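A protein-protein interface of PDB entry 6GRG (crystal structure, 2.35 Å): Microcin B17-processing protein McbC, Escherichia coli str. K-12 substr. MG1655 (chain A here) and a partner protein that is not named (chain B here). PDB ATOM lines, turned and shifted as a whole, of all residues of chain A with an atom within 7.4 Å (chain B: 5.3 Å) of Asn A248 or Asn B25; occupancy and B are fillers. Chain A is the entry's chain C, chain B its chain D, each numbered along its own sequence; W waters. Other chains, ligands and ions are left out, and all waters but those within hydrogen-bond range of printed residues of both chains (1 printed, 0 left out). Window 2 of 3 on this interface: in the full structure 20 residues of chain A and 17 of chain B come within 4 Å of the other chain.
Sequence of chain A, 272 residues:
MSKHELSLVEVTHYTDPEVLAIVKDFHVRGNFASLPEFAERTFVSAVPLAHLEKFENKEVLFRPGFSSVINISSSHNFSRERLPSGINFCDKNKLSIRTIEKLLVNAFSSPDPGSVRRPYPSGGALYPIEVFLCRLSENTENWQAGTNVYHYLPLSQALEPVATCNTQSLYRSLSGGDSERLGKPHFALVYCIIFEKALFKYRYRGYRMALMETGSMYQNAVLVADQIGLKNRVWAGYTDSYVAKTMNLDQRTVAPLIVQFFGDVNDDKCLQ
Asn A248 touches just these residues of chain B: Leu B22 (3.7 Å), Asn B23 (3.6 Å), Arg B24 (3.0 Å) and Asn B25 (3.2 Å).
Asn B25 touches just one residue of chain A: Asn A248.
Of the printed residues of chain A, Arg B24 touches Lys A245, Asn A248, Leu A249 and Asp A250.
Printed residues of chain B within 4 Å of Asp A250: Leu B22 (2.9 Å) and Arg B24 (3.8 Å).
Tyr A242 touches none of the printed residues of chain B.
Phe A132 touches none of the printed residues of chain B.
The nearest printed residue of chain B that does not touch Asn A248 is Asn B196 (6.2 Å).
The nearest residue of chain A that does not touch Asn B25 is Asp A250 (6.2 Å).
The nearest printed residue of chain A that does not touch Asn B23 is Asp A250 (4.3 Å).
The side-chain amide oxygen (OD1) of Asn B25 is in hydrogen-bond range of the side-chain amide nitrogen (ND2) of Asn B196 (3.1 Å).
OD1 of Asn B23 is in hydrogen-bond range of N of Asn B25 (3.0 Å).
The backbone NH of Leu A249 lies within hydrogen-bond range of the backbone carbonyl oxygen of Ala A244.
The side-chain amide nitrogen (ND2) of Asn B23 lies within hydrogen-bond range of the side-chain carboxylate (OE1) of Glu B200.
Printed residues of chain B that touch a printed residue of chain A: Leu B22, Asn B23, Arg B24 and Asn B25.
Hydrophobic or aromatic side chains of chain B that line the printed part of chain A: Leu B22.
N of Arg B24 lies within hydrogen-bond range of O of Asn A248 (3.0 Å).
The side-chain amide nitrogen (ND2) of Asn B25 lies within hydrogen-bond range of the side-chain amide oxygen (OD1) of Asn A248, 3.2 Å away.
The backbone NH of Asp A250 sits at hydrogen-bond distance from the backbone carbonyl oxygen of Leu B22.
Water W1 lies within hydrogen-bond range of the backbone carbonyl oxygen (O) of Lys A245 (2.7 Å), the side-chain amide oxygen (OD1) of Asn A248 (3.0 Å) and the guanidinium group (NH2) of Arg B24 (3.2 Å).
Lys A245 touches Arg B24 (CE to NH2, 3.6 Å).
O of Asn A248 touches O of Leu B22, at 3.7 Å.
Asn A248 touches Asn B23 (O to CA, 3.6 Å).
Leu B22 touches Leu A249 (O to CA, 3.2 Å).
Arg B24 touches Leu A249.
Arg B24 touches Asp A250 (CA to CB, 3.8 Å).
CG1 of Val A254 touches O of Leu B22, 3.8 Å away.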
ATOM      1  N   PHE A 132     -25.523 -19.653 -15.574  1.00  0.00           N
ATOM      2  CA  PHE A 132     -24.172 -19.354 -16.014  1.00  0.00           C
ATOM      3  C   PHE A 132     -24.245 -18.263 -17.079  1.00  0.00           C
ATOM      4  O   PHE A 132     -25.221 -18.175 -17.803  1.00  0.00           O
ATOM      5  CB  PHE A 132     -23.467 -20.616 -16.510  1.00  0.00           C
ATOM      6  CG  PHE A 132     -23.042 -21.580 -15.428  1.00  0.00           C
ATOM      7  CD1 PHE A 132     -23.911 -22.551 -14.960  1.00  0.00           C
ATOM      8  CD2 PHE A 132     -21.767 -21.518 -14.871  1.00  0.00           C
ATOM      9  CE1 PHE A 132     -23.520 -23.443 -13.971  1.00  0.00           C
ATOM     10  CE2 PHE A 132     -21.379 -22.408 -13.882  1.00  0.00           C
ATOM     11  CZ  PHE A 132     -22.258 -23.366 -13.430  1.00  0.00           C
ATOM     12  N   VAL A 149     -16.760 -17.301 -19.073  1.00  0.00           N
ATOM     13  CA  VAL A 149     -17.853 -17.977 -18.400  1.00  0.00           C
ATOM     14  C   VAL A 149     -17.836 -17.560 -16.935  1.00  0.00           C
ATOM     15  O   VAL A 149     -16.807 -17.501 -16.320  1.00  0.00           O
ATOM     16  CB  VAL A 149     -17.807 -19.504 -18.558  1.00  0.00           C
ATOM     17  CG1 VAL A 149     -19.120 -20.120 -18.117  1.00  0.00           C
ATOM     18  CG2 VAL A 149     -17.487 -19.913 -19.987  1.00  0.00           C
ATOM     19  N   VAL A 162     -15.647 -19.000 -14.083  1.00  0.00           N
ATOM     20  CA  VAL A 162     -15.830 -20.406 -14.365  1.00  0.00           C
ATOM     21  C   VAL A 162     -14.773 -20.875 -15.373  1.00  0.00           C
ATOM     22  O   VAL A 162     -14.164 -21.916 -15.164  1.00  0.00           O
ATOM     23  CB  VAL A 162     -17.280 -20.666 -14.825  1.00  0.00           C
ATOM     24  CG1 VAL A 162     -17.489 -22.079 -15.340  1.00  0.00           C
ATOM     25  CG2 VAL A 162     -18.248 -20.358 -13.700  1.00  0.00           C
ATOM     26  N   ALA A 163     -14.570 -20.124 -16.462  1.00  0.00           N
ATOM     27  CA  ALA A 163     -13.775 -20.602 -17.592  1.00  0.00           C
ATOM     28  C   ALA A 163     -13.175 -19.438 -18.383  1.00  0.00           C
ATOM     29  O   ALA A 163     -13.799 -18.371 -18.569  1.00  0.00           O
ATOM     30  CB  ALA A 163     -14.622 -21.472 -18.494  1.00  0.00           C
ATOM     31  N   THR A 164     -11.971 -19.688 -18.896  1.00  0.00           N
ATOM     32  CA  THR A 164     -11.291 -18.743 -19.727  1.00  0.00           C
ATOM     33  C   THR A 164     -11.232 -19.262 -21.171  1.00  0.00           C
ATOM     34  O   THR A 164     -10.352 -18.877 -21.918  1.00  0.00           O
ATOM     35  CB  THR A 164      -9.885 -18.441 -19.192  1.00  0.00           C
ATOM     36  OG1 THR A 164      -9.112 -19.620 -19.428  1.00  0.00           O
ATOM     37  CG2 THR A 164      -9.865 -18.068 -17.725  1.00  0.00           C
ATOM     38  N   CYS A 165     -12.200 -20.080 -21.590  1.00  0.00           N
ATOM     39  CA  CYS A 165     -12.330 -20.371 -23.011  1.00  0.00           C
ATOM     40  C   CYS A 165     -12.497 -19.044 -23.763  1.00  0.00           C
ATOM     41  O   CYS A 165     -13.009 -18.044 -23.222  1.00  0.00           O
ATOM     42  CB  CYS A 165     -13.507 -21.291 -23.296  1.00  0.00           C
ATOM     43  SG  CYS A 165     -15.008 -20.821 -22.401  1.00  0.00           S
ATOM     44  N   TYR A 242     -21.223 -30.679 -25.308  1.00  0.00           N
ATOM     45  CA  TYR A 242     -20.193 -29.804 -25.829  1.00  0.00           C
ATOM     46  C   TYR A 242     -20.225 -28.454 -25.074  1.00  0.00           C
ATOM     47  O   TYR A 242     -19.181 -27.839 -24.822  1.00  0.00           O
ATOM     48  CB  TYR A 242     -20.408 -29.676 -27.341  1.00  0.00           C
ATOM     49  CG  TYR A 242     -19.396 -28.859 -28.111  1.00  0.00           C
ATOM     50  CD1 TYR A 242     -18.059 -28.838 -27.754  1.00  0.00           C
ATOM     51  CD2 TYR A 242     -19.771 -28.134 -29.238  1.00  0.00           C
ATOM     52  CE1 TYR A 242     -17.130 -28.083 -28.452  1.00  0.00           C
ATOM     53  CE2 TYR A 242     -18.857 -27.378 -29.952  1.00  0.00           C
ATOM     54  CZ  TYR A 242     -17.532 -27.361 -29.553  1.00  0.00           C
ATOM     55  OH  TYR A 242     -16.599 -26.655 -30.235  1.00  0.00           O
ATOM     56  N   VAL A 243     -21.435 -27.981 -24.769  1.00  0.00           N
ATOM     57  CA  VAL A 243     -21.641 -26.765 -23.994  1.00  0.00           C
ATOM     58  C   VAL A 243     -21.056 -27.006 -22.603  1.00  0.00           C
ATOM     59  O   VAL A 243     -20.137 -26.298 -22.187  1.00  0.00           O
ATOM     60  CB  VAL A 243     -23.127 -26.376 -23.915  1.00  0.00           C
ATOM     61  CG1 VAL A 243     -23.385 -25.350 -22.824  1.00  0.00           C
ATOM     62  CG2 VAL A 243     -23.636 -25.851 -25.251  1.00  0.00           C
ATOM     63  N   ALA A 244     -21.566 -28.065 -21.963  1.00  0.00           N
ATOM     64  CA  ALA A 244     -21.077 -28.579 -20.691  1.00  0.00           C
ATOM     65  C   ALA A 244     -19.553 -28.595 -20.684  1.00  0.00           C
ATOM     66  O   ALA A 244     -18.953 -28.083 -19.772  1.00  0.00           O
ATOM     67  CB  ALA A 244     -21.606 -29.961 -20.434  1.00  0.00           C
ATOM     68  N   LYS A 245     -18.952 -29.186 -21.714  1.00  0.00           N
ATOM     69  CA  LYS A 245     -17.499 -29.394 -21.754  1.00  0.00           C
ATOM     70  C   LYS A 245     -16.788 -28.036 -21.710  1.00  0.00           C
ATOM     71  O   LYS A 245     -15.768 -27.874 -21.003  1.00  0.00           O
ATOM     72  CB  LYS A 245     -17.105 -30.160 -23.020  1.00  0.00           C
ATOM     73  CG  LYS A 245     -15.611 -30.223 -23.328  1.00  0.00           C
ATOM     74  CD  LYS A 245     -14.915 -31.391 -22.682  1.00  0.00           C
ATOM     75  CE  LYS A 245     -13.413 -31.286 -22.853  1.00  0.00           C
ATOM     76  NZ  LYS A 245     -12.771 -32.624 -22.870  1.00  0.00           N
ATOM     77  N   THR A 246     -17.361 -27.080 -22.457  1.00  0.00           N
ATOM     78  CA  THR A 246     -16.728 -25.814 -22.798  1.00  0.00           C
ATOM     79  C   THR A 246     -16.759 -24.888 -21.588  1.00  0.00           C
ATOM     80  O   THR A 246     -15.866 -24.069 -21.393  1.00  0.00           O
ATOM     81  CB  THR A 246     -17.425 -25.150 -23.990  1.00  0.00           C
ATOM     82  OG1 THR A 246     -17.352 -26.026 -25.118  1.00  0.00           O
ATOM     83  CG2 THR A 246     -16.792 -23.832 -24.368  1.00  0.00           C
ATOM     84  N   MET A 247     -17.817 -25.056 -20.796  1.00  0.00           N
ATOM     85  CA  MET A 247     -18.055 -24.331 -19.569  1.00  0.00           C
ATOM     86  C   MET A 247     -17.403 -25.020 -18.354  1.00  0.00           C
ATOM     87  O   MET A 247     -17.530 -24.539 -17.248  1.00  0.00           O
ATOM     88  CB  MET A 247     -19.565 -24.255 -19.355  1.00  0.00           C
ATOM     89  CG  MET A 247     -20.223 -23.238 -20.265  1.00  0.00           C
ATOM     90  SD  MET A 247     -22.003 -23.334 -20.072  1.00  0.00           S
ATOM     91  CE  MET A 247     -22.210 -22.416 -18.551  1.00  0.00           C
ATOM     92  N   ASN A 248     -16.757 -26.172 -18.579  1.00  0.00           N
ATOM     93  CA  ASN A 248     -16.051 -26.967 -17.573  1.00  0.00           C
ATOM     94  C   ASN A 248     -17.024 -27.483 -16.493  1.00  0.00           C
ATOM     95  O   ASN A 248     -16.639 -27.718 -15.369  1.00  0.00           O
ATOM     96  CB  ASN A 248     -14.839 -26.199 -17.024  1.00  0.00           C
ATOM     97  CG  ASN A 248     -13.657 -26.145 -17.978  1.00  0.00           C
ATOM     98  OD1 ASN A 248     -13.261 -27.145 -18.564  1.00  0.00           O
ATOM     99  ND2 ASN A 248     -13.054 -24.981 -18.116  1.00  0.00           N
ATOM    100  N   LEU A 249     -18.282 -27.711 -16.858  1.00  0.00           N
ATOM    101  CA  LEU A 249     -19.238 -28.426 -16.012  1.00  0.00           C
ATOM    102  C   LEU A 249     -18.937 -29.931 -16.076  1.00  0.00           C
ATOM    103  O   LEU A 249     -18.540 -30.446 -17.089  1.00  0.00           O
ATOM    104  CB  LEU A 249     -20.671 -28.164 -16.486  1.00  0.00           C
ATOM    105  CG  LEU A 249     -21.092 -26.704 -16.674  1.00  0.00           C
ATOM    106  CD1 LEU A 249     -22.522 -26.637 -17.191  1.00  0.00           C
ATOM    107  CD2 LEU A 249     -20.970 -25.895 -15.394  1.00  0.00           C
ATOM    108  N   ASP A 250     -19.116 -30.608 -14.947  1.00  0.00           N
ATOM    109  CA  ASP A 250     -19.042 -32.021 -14.845  1.00  0.00           C
ATOM    110  C   ASP A 250     -20.449 -32.570 -15.108  1.00  0.00           C
ATOM    111  O   ASP A 250     -21.372 -32.368 -14.312  1.00  0.00           O
ATOM    112  CB  ASP A 250     -18.521 -32.400 -13.465  1.00  0.00           C
ATOM    113  CG  ASP A 250     -18.256 -33.883 -13.274  1.00  0.00           C
ATOM    114  OD1 ASP A 250     -18.746 -34.697 -14.099  1.00  0.00           O
ATOM    115  OD2 ASP A 250     -17.562 -34.221 -12.287  1.00  0.00           O
ATOM    116  N   GLN A 251     -20.598 -33.291 -16.226  1.00  0.00           N
ATOM    117  CA  GLN A 251     -21.902 -33.769 -16.699  1.00  0.00           C
ATOM    118  C   GLN A 251     -22.501 -34.849 -15.776  1.00  0.00           C
ATOM    119  O   GLN A 251     -23.669 -35.149 -15.903  1.00  0.00           O
ATOM    120  CB  GLN A 251     -21.782 -34.311 -18.129  1.00  0.00           C
ATOM    121  CG  GLN A 251     -21.163 -33.319 -19.104  1.00  0.00           C
ATOM    122  CD  GLN A 251     -21.228 -33.825 -20.524  1.00  0.00           C
ATOM    123  OE1 GLN A 251     -22.273 -34.261 -20.989  1.00  0.00           O
ATOM    124  NE2 GLN A 251     -20.106 -33.774 -21.223  1.00  0.00           N
ATOM    125  N   VAL A 254     -24.230 -32.064 -13.292  1.00  0.00           N
ATOM    126  CA  VAL A 254     -24.938 -30.888 -13.779  1.00  0.00           C
ATOM    127  C   VAL A 254     -25.010 -30.932 -15.308  1.00  0.00           C
ATOM    128  O   VAL A 254     -24.082 -31.358 -15.939  1.00  0.00           O
ATOM    129  CB  VAL A 254     -24.265 -29.588 -13.293  1.00  0.00           C
ATOM    130  CG1 VAL A 254     -22.771 -29.523 -13.625  1.00  0.00           C
ATOM    131  CG2 VAL A 254     -24.971 -28.349 -13.820  1.00  0.00           C
ATOM    132  N   LEU B  22     -19.912 -29.224  -9.423  1.00  0.00           N
ATOM    133  CA  LEU B  22     -20.190 -28.498 -10.662  1.00  0.00           C
ATOM    134  C   LEU B  22     -18.992 -28.544 -11.614  1.00  0.00           C
ATOM    135  O   LEU B  22     -19.182 -28.660 -12.808  1.00  0.00           O
ATOM    136  CB  LEU B  22     -20.522 -27.045 -10.340  1.00  0.00           C
ATOM    137  CG  LEU B  22     -21.826 -26.813  -9.591  1.00  0.00           C
ATOM    138  CD1 LEU B  22     -22.203 -25.334  -9.634  1.00  0.00           C
ATOM    139  CD2 LEU B  22     -22.944 -27.669 -10.172  1.00  0.00           C
ATOM    140  N   ASN B  23     -17.780 -28.408 -11.062  1.00  0.00           N
ATOM    141  CA  ASN B  23     -16.536 -28.109 -11.783  1.00  0.00           C
ATOM    142  C   ASN B  23     -15.792 -29.412 -12.111  1.00  0.00           C
ATOM    143  O   ASN B  23     -15.425 -30.171 -11.199  1.00  0.00           O
ATOM    144  CB  ASN B  23     -15.678 -27.181 -10.927  1.00  0.00           C
ATOM    145  CG  ASN B  23     -14.423 -26.735 -11.639  1.00  0.00           C
ATOM    146  OD1 ASN B  23     -14.145 -27.209 -12.739  1.00  0.00           O
ATOM    147  ND2 ASN B  23     -13.680 -25.824 -11.032  1.00  0.00           N
ATOM    148  N   ARG B  24     -15.553 -29.675 -13.402  1.00  0.00           N
ATOM    149  CA  ARG B  24     -15.004 -30.971 -13.828  1.00  0.00           C
ATOM    150  C   ARG B  24     -13.497 -31.011 -13.576  1.00  0.00           C
ATOM    151  O   ARG B  24     -12.921 -32.095 -13.576  1.00  0.00           O
ATOM    152  CB  ARG B  24     -15.265 -31.253 -15.308  1.00  0.00           C
ATOM    153  CG  ARG B  24     -14.302 -30.581 -16.278  1.00  0.00           C
ATOM    154  CD  ARG B  24     -14.710 -30.838 -17.726  1.00  0.00           C
ATOM    155  NE  ARG B  24     -13.899 -30.149 -18.715  1.00  0.00           N
ATOM    156  CZ  ARG B  24     -12.663 -30.504 -19.052  1.00  0.00           C
ATOM    157  NH1 ARG B  24     -12.096 -31.576 -18.508  1.00  0.00           N
ATOM    158  NH2 ARG B  24     -12.003 -29.766 -19.929  1.00  0.00           N
ATOM    159  N   ASN B  25     -12.887 -29.828 -13.405  1.00  0.00           N
ATOM    160  CA  ASN B  25     -11.469 -29.701 -13.144  1.00  0.00           C
ATOM    161  C   ASN B  25     -11.167 -29.689 -11.632  1.00  0.00           C
ATOM    162  O   ASN B  25     -10.020 -29.574 -11.266  1.00  0.00           O
ATOM    163  CB  ASN B  25     -10.906 -28.448 -13.820  1.00  0.00           C
ATOM    164  CG  ASN B  25     -10.924 -28.541 -15.328  1.00  0.00           C
ATOM    165  OD1 ASN B  25     -10.466 -29.538 -15.874  1.00  0.00           O
ATOM    166  ND2 ASN B  25     -11.457 -27.530 -16.006  1.00  0.00           N
ATOM    167  N   MET B  26     -12.185 -29.731 -10.760  1.00  0.00           N
ATOM    168  CA  MET B  26     -11.981 -29.927  -9.312  1.00  0.00           C
ATOM    169  C   MET B  26     -11.826 -31.418  -9.033  1.00  0.00           C
ATOM    170  O   MET B  26     -12.353 -32.251  -9.764  1.00  0.00           O
ATOM    171  CB  MET B  26     -13.160 -29.391  -8.491  1.00  0.00           C
ATOM    172  CG  MET B  26     -13.086 -27.884  -8.161  1.00  0.00           C
ATOM    173  SD  MET B  26     -11.532 -27.286  -7.375  1.00  0.00           S
ATOM    174  CE  MET B  26     -12.186 -26.006  -6.298  1.00  0.00           C
ATOM    175  N   PRO B  27     -11.127 -31.828  -7.956  1.00  0.00           N
ATOM    176  CA  PRO B  27     -11.024 -33.249  -7.626  1.00  0.00           C
ATOM    177  C   PRO B  27     -12.333 -33.817  -7.063  1.00  0.00           C
ATOM    178  O   PRO B  27     -13.108 -33.131  -6.415  1.00  0.00           O
ATOM    179  CB  PRO B  27      -9.952 -33.274  -6.534  1.00  0.00           C
ATOM    180  CG  PRO B  27     -10.129 -31.933  -5.847  1.00  0.00           C
ATOM    181  CD  PRO B  27     -10.459 -30.968  -6.969  1.00  0.00           C
ATOM    182  N   ASN B 196      -4.743 -31.127 -14.407  1.00  0.00           N
ATOM    183  CA  ASN B 196      -5.810 -30.153 -14.334  1.00  0.00           C
ATOM    184  C   ASN B 196      -6.215 -29.877 -12.881  1.00  0.00           C
ATOM    185  O   ASN B 196      -6.235 -28.695 -12.489  1.00  0.00           O
ATOM    186  CB  ASN B 196      -7.025 -30.569 -15.167  1.00  0.00           C
ATOM    187  CG  ASN B 196      -6.873 -30.143 -16.608  1.00  0.00           C
ATOM    188  OD1 ASN B 196      -6.058 -30.706 -17.331  1.00  0.00           O
ATOM    189  ND2 ASN B 196      -7.607 -29.118 -17.018  1.00  0.00           N
ATOM    190  N   HIS B 197      -6.548 -30.927 -12.109  1.00  0.00           N
ATOM    191  CA  HIS B 197      -7.186 -30.717 -10.790  1.00  0.00           C
ATOM    192  C   HIS B 197      -6.195 -30.149  -9.770  1.00  0.00           C
ATOM    193  O   HIS B 197      -6.607 -29.439  -8.860  1.00  0.00           O
ATOM    194  CB  HIS B 197      -7.918 -31.955 -10.249  1.00  0.00           C
ATOM    195  CG  HIS B 197      -7.063 -33.134  -9.926  1.00  0.00           C
ATOM    196  ND1 HIS B 197      -6.780 -34.119 -10.858  1.00  0.00           N
ATOM    197  CD2 HIS B 197      -6.507 -33.542  -8.766  1.00  0.00           C
ATOM    198  CE1 HIS B 197      -6.075 -35.073 -10.291  1.00  0.00           C
ATOM    199  NE2 HIS B 197      -5.882 -34.739  -9.012  1.00  0.00           N
ATOM    200  N   GLU B 200      -5.925 -26.393 -10.611  1.00  0.00           N
ATOM    201  CA  GLU B 200      -7.187 -25.773 -10.161  1.00  0.00           C
ATOM    202  C   GLU B 200      -7.108 -25.377  -8.684  1.00  0.00           C
ATOM    203  O   GLU B 200      -7.460 -24.239  -8.307  1.00  0.00           O
ATOM    204  CB  GLU B 200      -8.379 -26.728 -10.237  1.00  0.00           C
ATOM    205  CG  GLU B 200      -9.176 -26.667 -11.522  1.00  0.00           C
ATOM    206  CD  GLU B 200      -9.827 -25.362 -11.952  1.00  0.00           C
ATOM    207  OE1 GLU B 200     -10.880 -24.996 -11.382  1.00  0.00           O
ATOM    208  OE2 GLU B 200      -9.320 -24.764 -12.926  1.00  0.00           O
HETATM  209  O   HOH W   1     -13.184 -27.289 -21.551  1.00  0.00           O
